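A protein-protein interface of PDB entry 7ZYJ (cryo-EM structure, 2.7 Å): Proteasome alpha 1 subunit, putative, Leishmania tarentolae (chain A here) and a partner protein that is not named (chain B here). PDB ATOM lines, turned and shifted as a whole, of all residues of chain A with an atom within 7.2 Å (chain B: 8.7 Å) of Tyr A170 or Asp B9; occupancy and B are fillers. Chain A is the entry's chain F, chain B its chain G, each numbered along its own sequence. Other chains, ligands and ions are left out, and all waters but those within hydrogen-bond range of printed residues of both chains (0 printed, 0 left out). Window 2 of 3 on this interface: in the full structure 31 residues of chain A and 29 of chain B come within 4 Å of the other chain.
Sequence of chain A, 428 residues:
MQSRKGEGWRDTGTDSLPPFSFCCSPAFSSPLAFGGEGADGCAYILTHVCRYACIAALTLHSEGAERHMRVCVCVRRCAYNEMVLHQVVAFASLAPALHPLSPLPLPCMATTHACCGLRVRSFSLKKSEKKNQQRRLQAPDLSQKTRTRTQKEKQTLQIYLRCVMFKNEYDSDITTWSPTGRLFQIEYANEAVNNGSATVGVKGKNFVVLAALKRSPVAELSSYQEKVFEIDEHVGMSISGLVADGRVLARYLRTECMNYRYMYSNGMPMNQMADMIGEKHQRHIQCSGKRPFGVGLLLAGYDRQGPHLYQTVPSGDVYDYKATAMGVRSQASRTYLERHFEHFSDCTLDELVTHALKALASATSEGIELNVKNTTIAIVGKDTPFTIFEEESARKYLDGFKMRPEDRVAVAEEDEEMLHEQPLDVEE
Among the printed residues, merely in contact across the chains: Ser A178 with Tyr B26 (3.3 Å), Trp A177 with Tyr B26 (3.3 Å), Tyr A170 with Gln B10 (3.5 Å), Thr A176 with Gln B23 (3.5 Å), Thr A175 with Gln B23 (3.6 Å) and Pro A179 with Tyr B26 (3.7 Å).
The side-chain carboxylate (OD2) of Asp B9 sits at hydrogen-bond distance from the side-chain hydroxyl (OH) of Tyr B26, 3.0 Å away. The side-chain amide nitrogen (NE2) of Gln B23 lies within hydrogen-bond range of the backbone carbonyl oxygen (O) of Asp B9 (2.5 Å). OD1 of Asn A168 is in hydrogen-bond range of N of Tyr A170, at 3.3 Å. OD1 of Asp B9 is in hydrogen-bond range of NE2 of Gln B10 (3.4 Å). O of Ser B6 is in hydrogen-bond range of NE2 of Gln B10 (3.4 Å).
The backbone NH (N) of Trp A177 sits at hydrogen-bond distance from the side-chain amide oxygen (OE1) of Gln B23 (2.6 Å). OD2 of Asp B9 is in hydrogen-bond range of OH of Tyr A170 (2.4 Å). The side-chain hydroxyl (OG1) of Thr A176 is in hydrogen-bond range of the backbone carbonyl oxygen (O) of Gln B10 (3.5 Å). O of Glu A169 lies close to OE1 of Gln B10, 3.1 Å away.
Printed residues of chain B that touch a printed residue of chain A: Asp B9, Gln B10, Gln B23 and Tyr B26. Hydrophobic or aromatic side chains of chain B that line the printed part of chain A: Tyr B26. Of the 17 printed residues of chain A, 7 touch a printed residue of chain B. Printed residues of chain A that touch a printed residue of chain B: Glu A169, Tyr A170, Thr A175, Thr A176, Trp A177, Ser A178 and Pro A179. Among the printed residues, 10 pairs touch across the chains. Among the printed residues, no Asp or Glu carboxylate lies within 4 Å of a Lys or Arg side-chain nitrogen of the other chain.
Printed residues of chain B within 4 Å of Tyr A170: Asp B9 and Gln B10. Printed residues of chain A within 4 Å of Asp B9: Tyr A170 (2.4 Å). Of the printed residues of chain A, Tyr B26 touches Trp A177, Ser A178 and Pro A179. Of the printed residues of chain B, Pro A179 touches Tyr B26 (3.7 Å). Printed residues of chain A within 4 Å of Gln B23: Thr A175 (3.6 Å), Thr A176 (3.5 Å) and Trp A177 (2.6 Å). Of the printed residues of chain B, Glu A169 touches Gln B10 (3.1 Å). Of the printed residues of chain B, Ser A178 touches Tyr B26 (3.3 Å). Phe B22 touches none of the printed residues of chain A. The nearest residue of chain B that does not touch Tyr A170 is Tyr B26 (4.4 Å). The nearest printed residue of chain A that does not touch Asp B9 is Trp A177 (4.9 Å).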
ATOM      1  N   ASN A 168     -24.682  -0.901  25.668  1.00  0.00           N
ATOM      2  CA  ASN A 168     -23.415  -1.609  25.803  1.00  0.00           C
ATOM      3  C   ASN A 168     -23.070  -1.823  27.272  1.00  0.00           C
ATOM      4  O   ASN A 168     -22.894  -0.866  28.023  1.00  0.00           O
ATOM      5  CB  ASN A 168     -22.292  -0.840  25.104  1.00  0.00           C
ATOM      6  CG  ASN A 168     -21.088  -1.709  24.806  1.00  0.00           C
ATOM      7  OD1 ASN A 168     -21.053  -2.886  25.166  1.00  0.00           O
ATOM      8  ND2 ASN A 168     -20.092  -1.133  24.146  1.00  0.00           N
ATOM      9  N   GLU A 169     -22.971  -3.091  27.676  1.00  0.00           N
ATOM     10  CA  GLU A 169     -22.674  -3.449  29.058  1.00  0.00           C
ATOM     11  C   GLU A 169     -21.262  -4.002  29.216  1.00  0.00           C
ATOM     12  O   GLU A 169     -20.962  -4.645  30.227  1.00  0.00           O
ATOM     13  CB  GLU A 169     -23.700  -4.457  29.582  1.00  0.00           C
ATOM     14  CG  GLU A 169     -23.823  -5.714  28.740  1.00  0.00           C
ATOM     15  CD  GLU A 169     -24.842  -5.574  27.627  1.00  0.00           C
ATOM     16  OE1 GLU A 169     -25.379  -4.461  27.449  1.00  0.00           O
ATOM     17  OE2 GLU A 169     -25.106  -6.576  26.929  1.00  0.00           O
ATOM     18  N   TYR A 170     -20.389  -3.766  28.238  1.00  0.00           N
ATOM     19  CA  TYR A 170     -19.010  -4.238  28.286  1.00  0.00           C
ATOM     20  C   TYR A 170     -18.010  -3.097  28.149  1.00  0.00           C
ATOM     21  O   TYR A 170     -16.822  -3.342  27.919  1.00  0.00           O
ATOM     22  CB  TYR A 170     -18.769  -5.288  27.200  1.00  0.00           C
ATOM     23  CG  TYR A 170     -19.617  -6.528  27.351  1.00  0.00           C
ATOM     24  CD1 TYR A 170     -19.223  -7.566  28.185  1.00  0.00           C
ATOM     25  CD2 TYR A 170     -20.815  -6.660  26.662  1.00  0.00           C
ATOM     26  CE1 TYR A 170     -19.995  -8.699  28.327  1.00  0.00           C
ATOM     27  CE2 TYR A 170     -21.595  -7.791  26.799  1.00  0.00           C
ATOM     28  CZ  TYR A 170     -21.181  -8.807  27.631  1.00  0.00           C
ATOM     29  OH  TYR A 170     -21.954  -9.936  27.771  1.00  0.00           O
ATOM     30  N   ASP A 171     -18.465  -1.852  28.285  1.00  0.00           N
ATOM     31  CA  ASP A 171     -17.605  -0.689  28.126  1.00  0.00           C
ATOM     32  C   ASP A 171     -17.383   0.085  29.417  1.00  0.00           C
ATOM     33  O   ASP A 171     -16.656   1.085  29.402  1.00  0.00           O
ATOM     34  CB  ASP A 171     -18.183   0.255  27.063  1.00  0.00           C
ATOM     35  CG  ASP A 171     -19.603   0.686  27.372  1.00  0.00           C
ATOM     36  OD1 ASP A 171     -20.174   0.204  28.372  1.00  0.00           O
ATOM     37  OD2 ASP A 171     -20.150   1.511  26.612  1.00  0.00           O
ATOM     38  N   SER A 172     -17.981  -0.340  30.529  1.00  0.00           N
ATOM     39  CA  SER A 172     -17.885   0.409  31.774  1.00  0.00           C
ATOM     40  C   SER A 172     -16.650   0.064  32.595  1.00  0.00           C
ATOM     41  O   SER A 172     -16.381   0.747  33.588  1.00  0.00           O
ATOM     42  CB  SER A 172     -19.137   0.178  32.623  1.00  0.00           C
ATOM     43  OG  SER A 172     -19.207  -1.164  33.072  1.00  0.00           O
ATOM     44  N   ASP A 173     -15.897  -0.967  32.219  1.00  0.00           N
ATOM     45  CA  ASP A 173     -14.734  -1.379  32.988  1.00  0.00           C
ATOM     46  C   ASP A 173     -13.580  -1.689  32.048  1.00  0.00           C
ATOM     47  O   ASP A 173     -13.775  -2.050  30.885  1.00  0.00           O
ATOM     48  CB  ASP A 173     -15.045  -2.599  33.867  1.00  0.00           C
ATOM     49  CG  ASP A 173     -14.148  -2.681  35.086  1.00  0.00           C
ATOM     50  OD1 ASP A 173     -13.074  -2.043  35.082  1.00  0.00           O
ATOM     51  OD2 ASP A 173     -14.519  -3.381  36.051  1.00  0.00           O
ATOM     52  N   ILE A 174     -12.363  -1.541  32.573  1.00  0.00           N
ATOM     53  CA  ILE A 174     -11.164  -1.856  31.806  1.00  0.00           C
ATOM     54  C   ILE A 174     -10.824  -3.343  31.811  1.00  0.00           C
ATOM     55  O   ILE A 174     -10.180  -3.823  30.868  1.00  0.00           O
ATOM     56  CB  ILE A 174      -9.959  -1.044  32.318  1.00  0.00           C
ATOM     57  CG1 ILE A 174      -8.902  -0.913  31.224  1.00  0.00           C
ATOM     58  CG2 ILE A 174      -9.373  -1.657  33.579  1.00  0.00           C
ATOM     59  CD1 ILE A 174      -7.944   0.208  31.455  1.00  0.00           C
ATOM     60  N   THR A 175     -11.239  -4.087  32.837  1.00  0.00           N
ATOM     61  CA  THR A 175     -10.959  -5.513  32.933  1.00  0.00           C
ATOM     62  C   THR A 175     -12.102  -6.361  32.391  1.00  0.00           C
ATOM     63  O   THR A 175     -12.262  -7.518  32.793  1.00  0.00           O
ATOM     64  CB  THR A 175     -10.655  -5.902  34.380  1.00  0.00           C
ATOM     65  OG1 THR A 175     -11.811  -5.669  35.194  1.00  0.00           O
ATOM     66  CG2 THR A 175      -9.487  -5.094  34.916  1.00  0.00           C
ATOM     67  N   THR A 176     -12.902  -5.806  31.485  1.00  0.00           N
ATOM     68  CA  THR A 176     -14.033  -6.510  30.895  1.00  0.00           C
ATOM     69  C   THR A 176     -13.769  -6.700  29.410  1.00  0.00           C
ATOM     70  O   THR A 176     -13.550  -5.723  28.684  1.00  0.00           O
ATOM     71  CB  THR A 176     -15.337  -5.741  31.113  1.00  0.00           C
ATOM     72  OG1 THR A 176     -15.597  -5.626  32.517  1.00  0.00           O
ATOM     73  CG2 THR A 176     -16.498  -6.462  30.447  1.00  0.00           C
ATOM     74  N   TRP A 177     -13.785  -7.952  28.964  1.00  0.00           N
ATOM     75  CA  TRP A 177     -13.651  -8.274  27.553  1.00  0.00           C
ATOM     76  C   TRP A 177     -15.014  -8.253  26.878  1.00  0.00           C
ATOM     77  O   TRP A 177     -15.987  -8.803  27.401  1.00  0.00           O
ATOM     78  CB  TRP A 177     -13.006  -9.650  27.368  1.00  0.00           C
ATOM     79  CG  TRP A 177     -11.519  -9.671  27.535  1.00  0.00           C
ATOM     80  CD1 TRP A 177     -10.823 -10.080  28.633  1.00  0.00           C
ATOM     81  CD2 TRP A 177     -10.543  -9.290  26.560  1.00  0.00           C
ATOM     82  NE1 TRP A 177      -9.475  -9.966  28.408  1.00  0.00           N
ATOM     83  CE2 TRP A 177      -9.275  -9.483  27.143  1.00  0.00           C
ATOM     84  CE3 TRP A 177     -10.616  -8.798  25.254  1.00  0.00           C
ATOM     85  CZ2 TRP A 177      -8.092  -9.203  26.464  1.00  0.00           C
ATOM     86  CZ3 TRP A 177      -9.442  -8.520  24.583  1.00  0.00           C
ATOM     87  CH2 TRP A 177      -8.196  -8.722  25.188  1.00  0.00           C
ATOM     88  N   SER A 178     -15.079  -7.613  25.719  1.00  0.00           N
ATOM     89  CA  SER A 178     -16.281  -7.682  24.909  1.00  0.00           C
ATOM     90  C   SER A 178     -16.464  -9.103  24.377  1.00  0.00           C
ATOM     91  O   SER A 178     -15.484  -9.823  24.168  1.00  0.00           O
ATOM     92  CB  SER A 178     -16.197  -6.696  23.749  1.00  0.00           C
ATOM     93  OG  SER A 178     -17.344  -6.761  22.920  1.00  0.00           O
ATOM     94  N   PRO A 179     -17.709  -9.535  24.158  1.00  0.00           N
ATOM     95  CA  PRO A 179     -17.930 -10.885  23.612  1.00  0.00           C
ATOM     96  C   PRO A 179     -17.301 -11.102  22.248  1.00  0.00           C
ATOM     97  O   PRO A 179     -17.060 -12.257  21.877  1.00  0.00           O
ATOM     98  CB  PRO A 179     -19.459 -10.992  23.544  1.00  0.00           C
ATOM     99  CG  PRO A 179     -19.946 -10.020  24.559  1.00  0.00           C
ATOM    100  CD  PRO A 179     -18.974  -8.881  24.529  1.00  0.00           C
ATOM    101  N   ARG A 182     -13.050  -7.432  22.315  1.00  0.00           N
ATOM    102  CA  ARG A 182     -12.662  -6.032  22.264  1.00  0.00           C
ATOM    103  C   ARG A 182     -12.584  -5.464  23.673  1.00  0.00           C
ATOM    104  O   ARG A 182     -13.218  -5.970  24.602  1.00  0.00           O
ATOM    105  CB  ARG A 182     -13.647  -5.204  21.429  1.00  0.00           C
ATOM    106  CG  ARG A 182     -13.970  -5.803  20.073  1.00  0.00           C
ATOM    107  CD  ARG A 182     -15.059  -5.014  19.370  1.00  0.00           C
ATOM    108  NE  ARG A 182     -14.684  -3.620  19.170  1.00  0.00           N
ATOM    109  CZ  ARG A 182     -15.450  -2.719  18.571  1.00  0.00           C
ATOM    110  NH1 ARG A 182     -16.647  -3.031  18.102  1.00  0.00           N
ATOM    111  NH2 ARG A 182     -15.004  -1.473  18.440  1.00  0.00           N
ATOM    112  N   LEU A 183     -11.785  -4.415  23.822  1.00  0.00           N
ATOM    113  CA  LEU A 183     -11.680  -3.659  25.067  1.00  0.00           C
ATOM    114  C   LEU A 183     -12.127  -2.234  24.762  1.00  0.00           C
ATOM    115  O   LEU A 183     -11.391  -1.462  24.140  1.00  0.00           O
ATOM    116  CB  LEU A 183     -10.260  -3.707  25.617  1.00  0.00           C
ATOM    117  CG  LEU A 183      -9.727  -5.086  26.010  1.00  0.00           C
ATOM    118  CD1 LEU A 183      -8.221  -5.040  26.202  1.00  0.00           C
ATOM    119  CD2 LEU A 183     -10.415  -5.584  27.270  1.00  0.00           C
ATOM    120  N   PHE A 184     -13.337  -1.889  25.203  1.00  0.00           N
ATOM    121  CA  PHE A 184     -13.957  -0.643  24.765  1.00  0.00           C
ATOM    122  C   PHE A 184     -13.366   0.578  25.459  1.00  0.00           C
ATOM    123  O   PHE A 184     -13.382   1.673  24.889  1.00  0.00           O
ATOM    124  CB  PHE A 184     -15.466  -0.707  24.993  1.00  0.00           C
ATOM    125  CG  PHE A 184     -16.212  -1.386  23.883  1.00  0.00           C
ATOM    126  CD1 PHE A 184     -16.254  -0.830  22.616  1.00  0.00           C
ATOM    127  CD2 PHE A 184     -16.864  -2.587  24.103  1.00  0.00           C
ATOM    128  CE1 PHE A 184     -16.938  -1.456  21.591  1.00  0.00           C
ATOM    129  CE2 PHE A 184     -17.549  -3.218  23.083  1.00  0.00           C
ATOM    130  CZ  PHE A 184     -17.585  -2.652  21.826  1.00  0.00           C
ATOM    131  N   GLN A 185     -12.858   0.426  26.685  1.00  0.00           N
ATOM    132  CA  GLN A 185     -12.267   1.567  27.380  1.00  0.00           C
ATOM    133  C   GLN A 185     -11.021   2.068  26.658  1.00  0.00           C
ATOM    134  O   GLN A 185     -10.812   3.280  26.522  1.00  0.00           O
ATOM    135  CB  GLN A 185     -11.939   1.187  28.824  1.00  0.00           C
ATOM    136  CG  GLN A 185     -13.142   1.212  29.754  1.00  0.00           C
ATOM    137  CD  GLN A 185     -13.621   2.618  30.053  1.00  0.00           C
ATOM    138  OE1 GLN A 185     -12.911   3.408  30.675  1.00  0.00           O
ATOM    139  NE2 GLN A 185     -14.829   2.940  29.607  1.00  0.00           N
ATOM    140  N   TYR A 188     -12.131   3.962  23.679  1.00  0.00           N
ATOM    141  CA  TYR A 188     -12.550   5.303  24.073  1.00  0.00           C
ATOM    142  C   TYR A 188     -11.349   6.210  24.309  1.00  0.00           C
ATOM    143  O   TYR A 188     -11.385   7.398  23.969  1.00  0.00           O
ATOM    144  CB  TYR A 188     -13.423   5.232  25.325  1.00  0.00           C
ATOM    145  CG  TYR A 188     -14.741   4.515  25.123  1.00  0.00           C
ATOM    146  CD1 TYR A 188     -15.202   4.209  23.848  1.00  0.00           C
ATOM    147  CD2 TYR A 188     -15.522   4.140  26.207  1.00  0.00           C
ATOM    148  CE1 TYR A 188     -16.400   3.553  23.660  1.00  0.00           C
ATOM    149  CE2 TYR A 188     -16.724   3.485  26.028  1.00  0.00           C
ATOM    150  CZ  TYR A 188     -17.158   3.195  24.752  1.00  0.00           C
ATOM    151  OH  TYR A 188     -18.354   2.542  24.567  1.00  0.00           O
ATOM    152  N   SER B   6     -25.953 -11.674  30.889  1.00  0.00           N
ATOM    153  CA  SER B   6     -26.148 -11.173  32.244  1.00  0.00           C
ATOM    154  C   SER B   6     -24.816 -10.819  32.895  1.00  0.00           C
ATOM    155  O   SER B   6     -23.877 -10.394  32.222  1.00  0.00           O
ATOM    156  CB  SER B   6     -26.890 -12.205  33.095  1.00  0.00           C
ATOM    157  OG  SER B   6     -25.997 -13.178  33.607  1.00  0.00           O
ATOM    158  N   GLY B   7     -24.742 -10.996  34.210  1.00  0.00           N
ATOM    159  CA  GLY B   7     -23.543 -10.725  34.974  1.00  0.00           C
ATOM    160  C   GLY B   7     -22.600 -11.897  35.133  1.00  0.00           C
ATOM    161  O   GLY B   7     -21.655 -11.806  35.924  1.00  0.00           O
ATOM    162  N   HIS B   8     -22.822 -12.993  34.412  1.00  0.00           N
ATOM    163  CA  HIS B   8     -21.991 -14.185  34.519  1.00  0.00           C
ATOM    164  C   HIS B   8     -20.771 -14.145  33.607  1.00  0.00           C
ATOM    165  O   HIS B   8     -20.000 -15.110  33.592  1.00  0.00           O
ATOM    166  CB  HIS B   8     -22.823 -15.432  34.210  1.00  0.00           C
ATOM    167  CG  HIS B   8     -23.210 -15.558  32.769  1.00  0.00           C
ATOM    168  ND1 HIS B   8     -23.982 -14.618  32.121  1.00  0.00           N
ATOM    169  CD2 HIS B   8     -22.931 -16.513  31.851  1.00  0.00           C
ATOM    170  CE1 HIS B   8     -24.162 -14.988  30.866  1.00  0.00           C
ATOM    171  NE2 HIS B   8     -23.534 -16.135  30.676  1.00  0.00           N
ATOM    172  N   ASP B   9     -20.579 -13.062  32.852  1.00  0.00           N
ATOM    173  CA  ASP B   9     -19.469 -12.973  31.911  1.00  0.00           C
ATOM    174  C   ASP B   9     -18.738 -11.640  32.025  1.00  0.00           C
ATOM    175  O   ASP B   9     -18.051 -11.224  31.086  1.00  0.00           O
ATOM    176  CB  ASP B   9     -19.953 -13.182  30.474  1.00  0.00           C
ATOM    177  CG  ASP B   9     -20.958 -12.134  30.037  1.00  0.00           C
ATOM    178  OD1 ASP B   9     -21.505 -11.427  30.908  1.00  0.00           O
ATOM    179  OD2 ASP B   9     -21.203 -12.019  28.819  1.00  0.00           O
ATOM    180  N   GLN B  10     -18.871 -10.960  33.163  1.00  0.00           N
ATOM    181  CA  GLN B  10     -18.247  -9.659  33.351  1.00  0.00           C
ATOM    182  C   GLN B  10     -16.876  -9.730  34.009  1.00  0.00           C
ATOM    183  O   GLN B  10     -16.094  -8.784  33.872  1.00  0.00           O
ATOM    184  CB  GLN B  10     -19.156  -8.750  34.185  1.00  0.00           C
ATOM    185  CG  GLN B  10     -20.567  -8.624  33.637  1.00  0.00           C
ATOM    186  CD  GLN B  10     -20.643  -7.702  32.437  1.00  0.00           C
ATOM    187  OE1 GLN B  10     -19.970  -6.674  32.386  1.00  0.00           O
ATOM    188  NE2 GLN B  10     -21.466  -8.068  31.461  1.00  0.00           N
ATOM    189  N   SER B  11     -16.563 -10.820  34.708  1.00  0.00           N
ATOM    190  CA  SER B  11     -15.281 -10.959  35.380  1.00  0.00           C
ATOM    191  C   SER B  11     -14.836 -12.413  35.322  1.00  0.00           C
ATOM    192  O   SER B  11     -15.643 -13.326  35.138  1.00  0.00           O
ATOM    193  CB  SER B  11     -15.349 -10.479  36.835  1.00  0.00           C
ATOM    194  OG  SER B  11     -16.526 -10.942  37.471  1.00  0.00           O
ATOM    195  N   THR B  12     -13.527 -12.615  35.484  1.00  0.00           N
ATOM    196  CA  THR B  12     -12.945 -13.947  35.378  1.00  0.00           C
ATOM    197  C   THR B  12     -13.191 -14.807  36.608  1.00  0.00           C
ATOM    198  O   THR B  12     -13.116 -16.035  36.509  1.00  0.00           O
ATOM    199  CB  THR B  12     -11.439 -13.847  35.142  1.00  0.00           C
ATOM    200  OG1 THR B  12     -10.817 -13.230  36.275  1.00  0.00           O
ATOM    201  CG2 THR B  12     -11.167 -13.010  33.925  1.00  0.00           C
ATOM    202  N   ASP B  13     -13.480 -14.201  37.754  1.00  0.00           N
ATOM    203  CA  ASP B  13     -13.665 -14.944  38.992  1.00  0.00           C
ATOM    204  C   ASP B  13     -15.027 -15.617  39.085  1.00  0.00           C
ATOM    205  O   ASP B  13     -15.382 -16.115  40.158  1.00  0.00           O
ATOM    206  CB  ASP B  13     -13.463 -14.019  40.196  1.00  0.00           C
ATOM    207  CG  ASP B  13     -14.611 -13.050  40.384  1.00  0.00           C
ATOM    208  OD1 ASP B  13     -14.853 -12.231  39.475  1.00  0.00           O
ATOM    209  OD2 ASP B  13     -15.271 -13.106  41.444  1.00  0.00           O
ATOM    210  N   VAL B  14     -15.791 -15.654  37.995  1.00  0.00           N
ATOM    211  CA  VAL B  14     -17.150 -16.176  38.000  1.00  0.00           C
ATOM    212  C   VAL B  14     -17.222 -17.345  37.028  1.00  0.00           C
ATOM    213  O   VAL B  14     -16.845 -17.208  35.858  1.00  0.00           O
ATOM    214  CB  VAL B  14     -18.179 -15.099  37.620  1.00  0.00           C
ATOM    215  CG1 VAL B  14     -19.579 -15.689  37.576  1.00  0.00           C
ATOM    216  CG2 VAL B  14     -18.114 -13.936  38.594  1.00  0.00           C
ATOM    217  N   PHE B  15     -17.698 -18.488  37.511  1.00  0.00           N
ATOM    218  CA  PHE B  15     -18.014 -19.609  36.639  1.00  0.00           C
ATOM    219  C   PHE B  15     -19.424 -19.468  36.085  1.00  0.00           C
ATOM    220  O   PHE B  15     -20.322 -18.930  36.738  1.00  0.00           O
ATOM    221  CB  PHE B  15     -17.893 -20.937  37.388  1.00  0.00           C
ATOM    222  CG  PHE B  15     -16.503 -21.497  37.423  1.00  0.00           C
ATOM    223  CD1 PHE B  15     -15.898 -21.955  36.266  1.00  0.00           C
ATOM    224  CD2 PHE B  15     -15.808 -21.586  38.617  1.00  0.00           C
ATOM    225  CE1 PHE B  15     -14.623 -22.477  36.295  1.00  0.00           C
ATOM    226  CE2 PHE B  15     -14.532 -22.109  38.650  1.00  0.00           C
ATOM    227  CZ  PHE B  15     -13.938 -22.555  37.489  1.00  0.00           C
ATOM    228  N   SER B  16     -19.614 -19.959  34.865  1.00  0.00           N
ATOM    229  CA  SER B  16     -20.944 -20.010  34.287  1.00  0.00           C
ATOM    230  C   SER B  16     -21.692 -21.237  34.803  1.00  0.00           C
ATOM    231  O   SER B  16     -21.131 -22.100  35.483  1.00  0.00           O
ATOM    232  CB  SER B  16     -20.867 -20.029  32.762  1.00  0.00           C
ATOM    233  OG  SER B  16     -20.338 -21.255  32.295  1.00  0.00           O
ATOM    234  N   ARG B  20     -17.955 -22.703  32.755  1.00  0.00           N
ATOM    235  CA  ARG B  20     -17.080 -21.996  31.834  1.00  0.00           C
ATOM    236  C   ARG B  20     -16.714 -20.625  32.388  1.00  0.00           C
ATOM    237  O   ARG B  20     -17.449 -20.044  33.192  1.00  0.00           O
ATOM    238  CB  ARG B  20     -17.744 -21.833  30.465  1.00  0.00           C
ATOM    239  CG  ARG B  20     -18.182 -23.139  29.833  1.00  0.00           C
ATOM    240  CD  ARG B  20     -18.202 -23.032  28.322  1.00  0.00           C
ATOM    241  NE  ARG B  20     -19.451 -22.464  27.829  1.00  0.00           N
ATOM    242  CZ  ARG B  20     -19.601 -21.915  26.633  1.00  0.00           C
ATOM    243  NH1 ARG B  20     -18.594 -21.828  25.780  1.00  0.00           N
ATOM    244  NH2 ARG B  20     -20.791 -21.436  26.284  1.00  0.00           N
ATOM    245  N   VAL B  21     -15.567 -20.117  31.953  1.00  0.00           N
ATOM    246  CA  VAL B  21     -15.125 -18.762  32.261  1.00  0.00           C
ATOM    247  C   VAL B  21     -15.198 -17.981  30.955  1.00  0.00           C
ATOM    248  O   VAL B  21     -14.347 -18.140  30.073  1.00  0.00           O
ATOM    249  CB  VAL B  21     -13.716 -18.737  32.861  1.00  0.00           C
ATOM    250  CG1 VAL B  21     -13.394 -17.347  33.386  1.00  0.00           C
ATOM    251  CG2 VAL B  21     -13.592 -19.772  33.966  1.00  0.00           C
ATOM    252  N   PHE B  22     -16.218 -17.131  30.828  1.00  0.00           N
ATOM    253  CA  PHE B  22     -16.511 -16.514  29.539  1.00  0.00           C
ATOM    254  C   PHE B  22     -15.511 -15.424  29.177  1.00  0.00           C
ATOM    255  O   PHE B  22     -15.277 -15.179  27.990  1.00  0.00           O
ATOM    256  CB  PHE B  22     -17.932 -15.957  29.541  1.00  0.00           C
ATOM    257  CG  PHE B  22     -18.967 -16.947  29.095  1.00  0.00           C
ATOM    258  CD1 PHE B  22     -19.027 -17.357  27.775  1.00  0.00           C
ATOM    259  CD2 PHE B  22     -19.873 -17.474  29.997  1.00  0.00           C
ATOM    260  CE1 PHE B  22     -19.975 -18.270  27.362  1.00  0.00           C
ATOM    261  CE2 PHE B  22     -20.824 -18.389  29.590  1.00  0.00           C
ATOM    262  CZ  PHE B  22     -20.874 -18.787  28.271  1.00  0.00           C
ATOM    263  N   GLN B  23     -14.927 -14.749  30.170  1.00  0.00           N
ATOM    264  CA  GLN B  23     -13.952 -13.704  29.869  1.00  0.00           C
ATOM    265  C   GLN B  23     -12.712 -14.284  29.200  1.00  0.00           C
ATOM    266  O   GLN B  23     -12.148 -13.679  28.279  1.00  0.00           O
ATOM    267  CB  GLN B  23     -13.578 -12.955  31.146  1.00  0.00           C
ATOM    268  CG  GLN B  23     -14.636 -11.970  31.610  1.00  0.00           C
ATOM    269  CD  GLN B  23     -14.682 -10.722  30.754  1.00  0.00           C
ATOM    270  OE1 GLN B  23     -13.682 -10.022  30.604  1.00  0.00           O
ATOM    271  NE2 GLN B  23     -15.846 -10.438  30.185  1.00  0.00           N
ATOM    272  N   VAL B  24     -12.274 -15.460  29.651  1.00  0.00           N
ATOM    273  CA  VAL B  24     -11.154 -16.135  29.006  1.00  0.00           C
ATOM    274  C   VAL B  24     -11.504 -16.497  27.569  1.00  0.00           C
ATOM    275  O   VAL B  24     -10.671 -16.376  26.662  1.00  0.00           O
ATOM    276  CB  VAL B  24     -10.744 -17.375  29.818  1.00  0.00           C
ATOM    277  CG1 VAL B  24      -9.568 -18.056  29.164  1.00  0.00           C
ATOM    278  CG2 VAL B  24     -10.408 -16.983  31.245  1.00  0.00           C
ATOM    279  N   GLU B  25     -12.735 -16.956  27.337  1.00  0.00           N
ATOM    280  CA  GLU B  25     -13.165 -17.259  25.977  1.00  0.00           C
ATOM    281  C   GLU B  25     -13.196 -16.012  25.106  1.00  0.00           C
ATOM    282  O   GLU B  25     -12.860 -16.076  23.921  1.00  0.00           O
ATOM    283  CB  GLU B  25     -14.536 -17.929  25.999  1.00  0.00           C
ATOM    284  CG  GLU B  25     -14.560 -19.225  26.779  1.00  0.00           C
ATOM    285  CD  GLU B  25     -15.911 -19.898  26.744  1.00  0.00           C
ATOM    286  OE1 GLU B  25     -16.833 -19.350  26.105  1.00  0.00           O
ATOM    287  OE2 GLU B  25     -16.050 -20.976  27.356  1.00  0.00           O
ATOM    288  N   TYR B  26     -13.598 -14.871  25.669  1.00  0.00           N
ATOM    289  CA  TYR B  26     -13.581 -13.625  24.908  1.00  0.00           C
ATOM    290  C   TYR B  26     -12.156 -13.205  24.571  1.00  0.00           C
ATOM    291  O   TYR B  26     -11.889 -12.712  23.468  1.00  0.00           O
ATOM    292  CB  TYR B  26     -14.300 -12.524  25.688  1.00  0.00           C
ATOM    293  CG  TYR B  26     -15.758 -12.809  25.978  1.00  0.00           C
ATOM    294  CD1 TYR B  26     -16.445 -13.804  25.294  1.00  0.00           C
ATOM    295  CD2 TYR B  26     -16.447 -12.082  26.939  1.00  0.00           C
ATOM    296  CE1 TYR B  26     -17.774 -14.066  25.558  1.00  0.00           C
ATOM    297  CE2 TYR B  26     -17.778 -12.337  27.209  1.00  0.00           C
ATOM    298  CZ  TYR B  26     -18.435 -13.329  26.515  1.00  0.00           C
ATOM    299  OH  TYR B  26     -19.759 -13.588  26.780  1.00  0.00           O
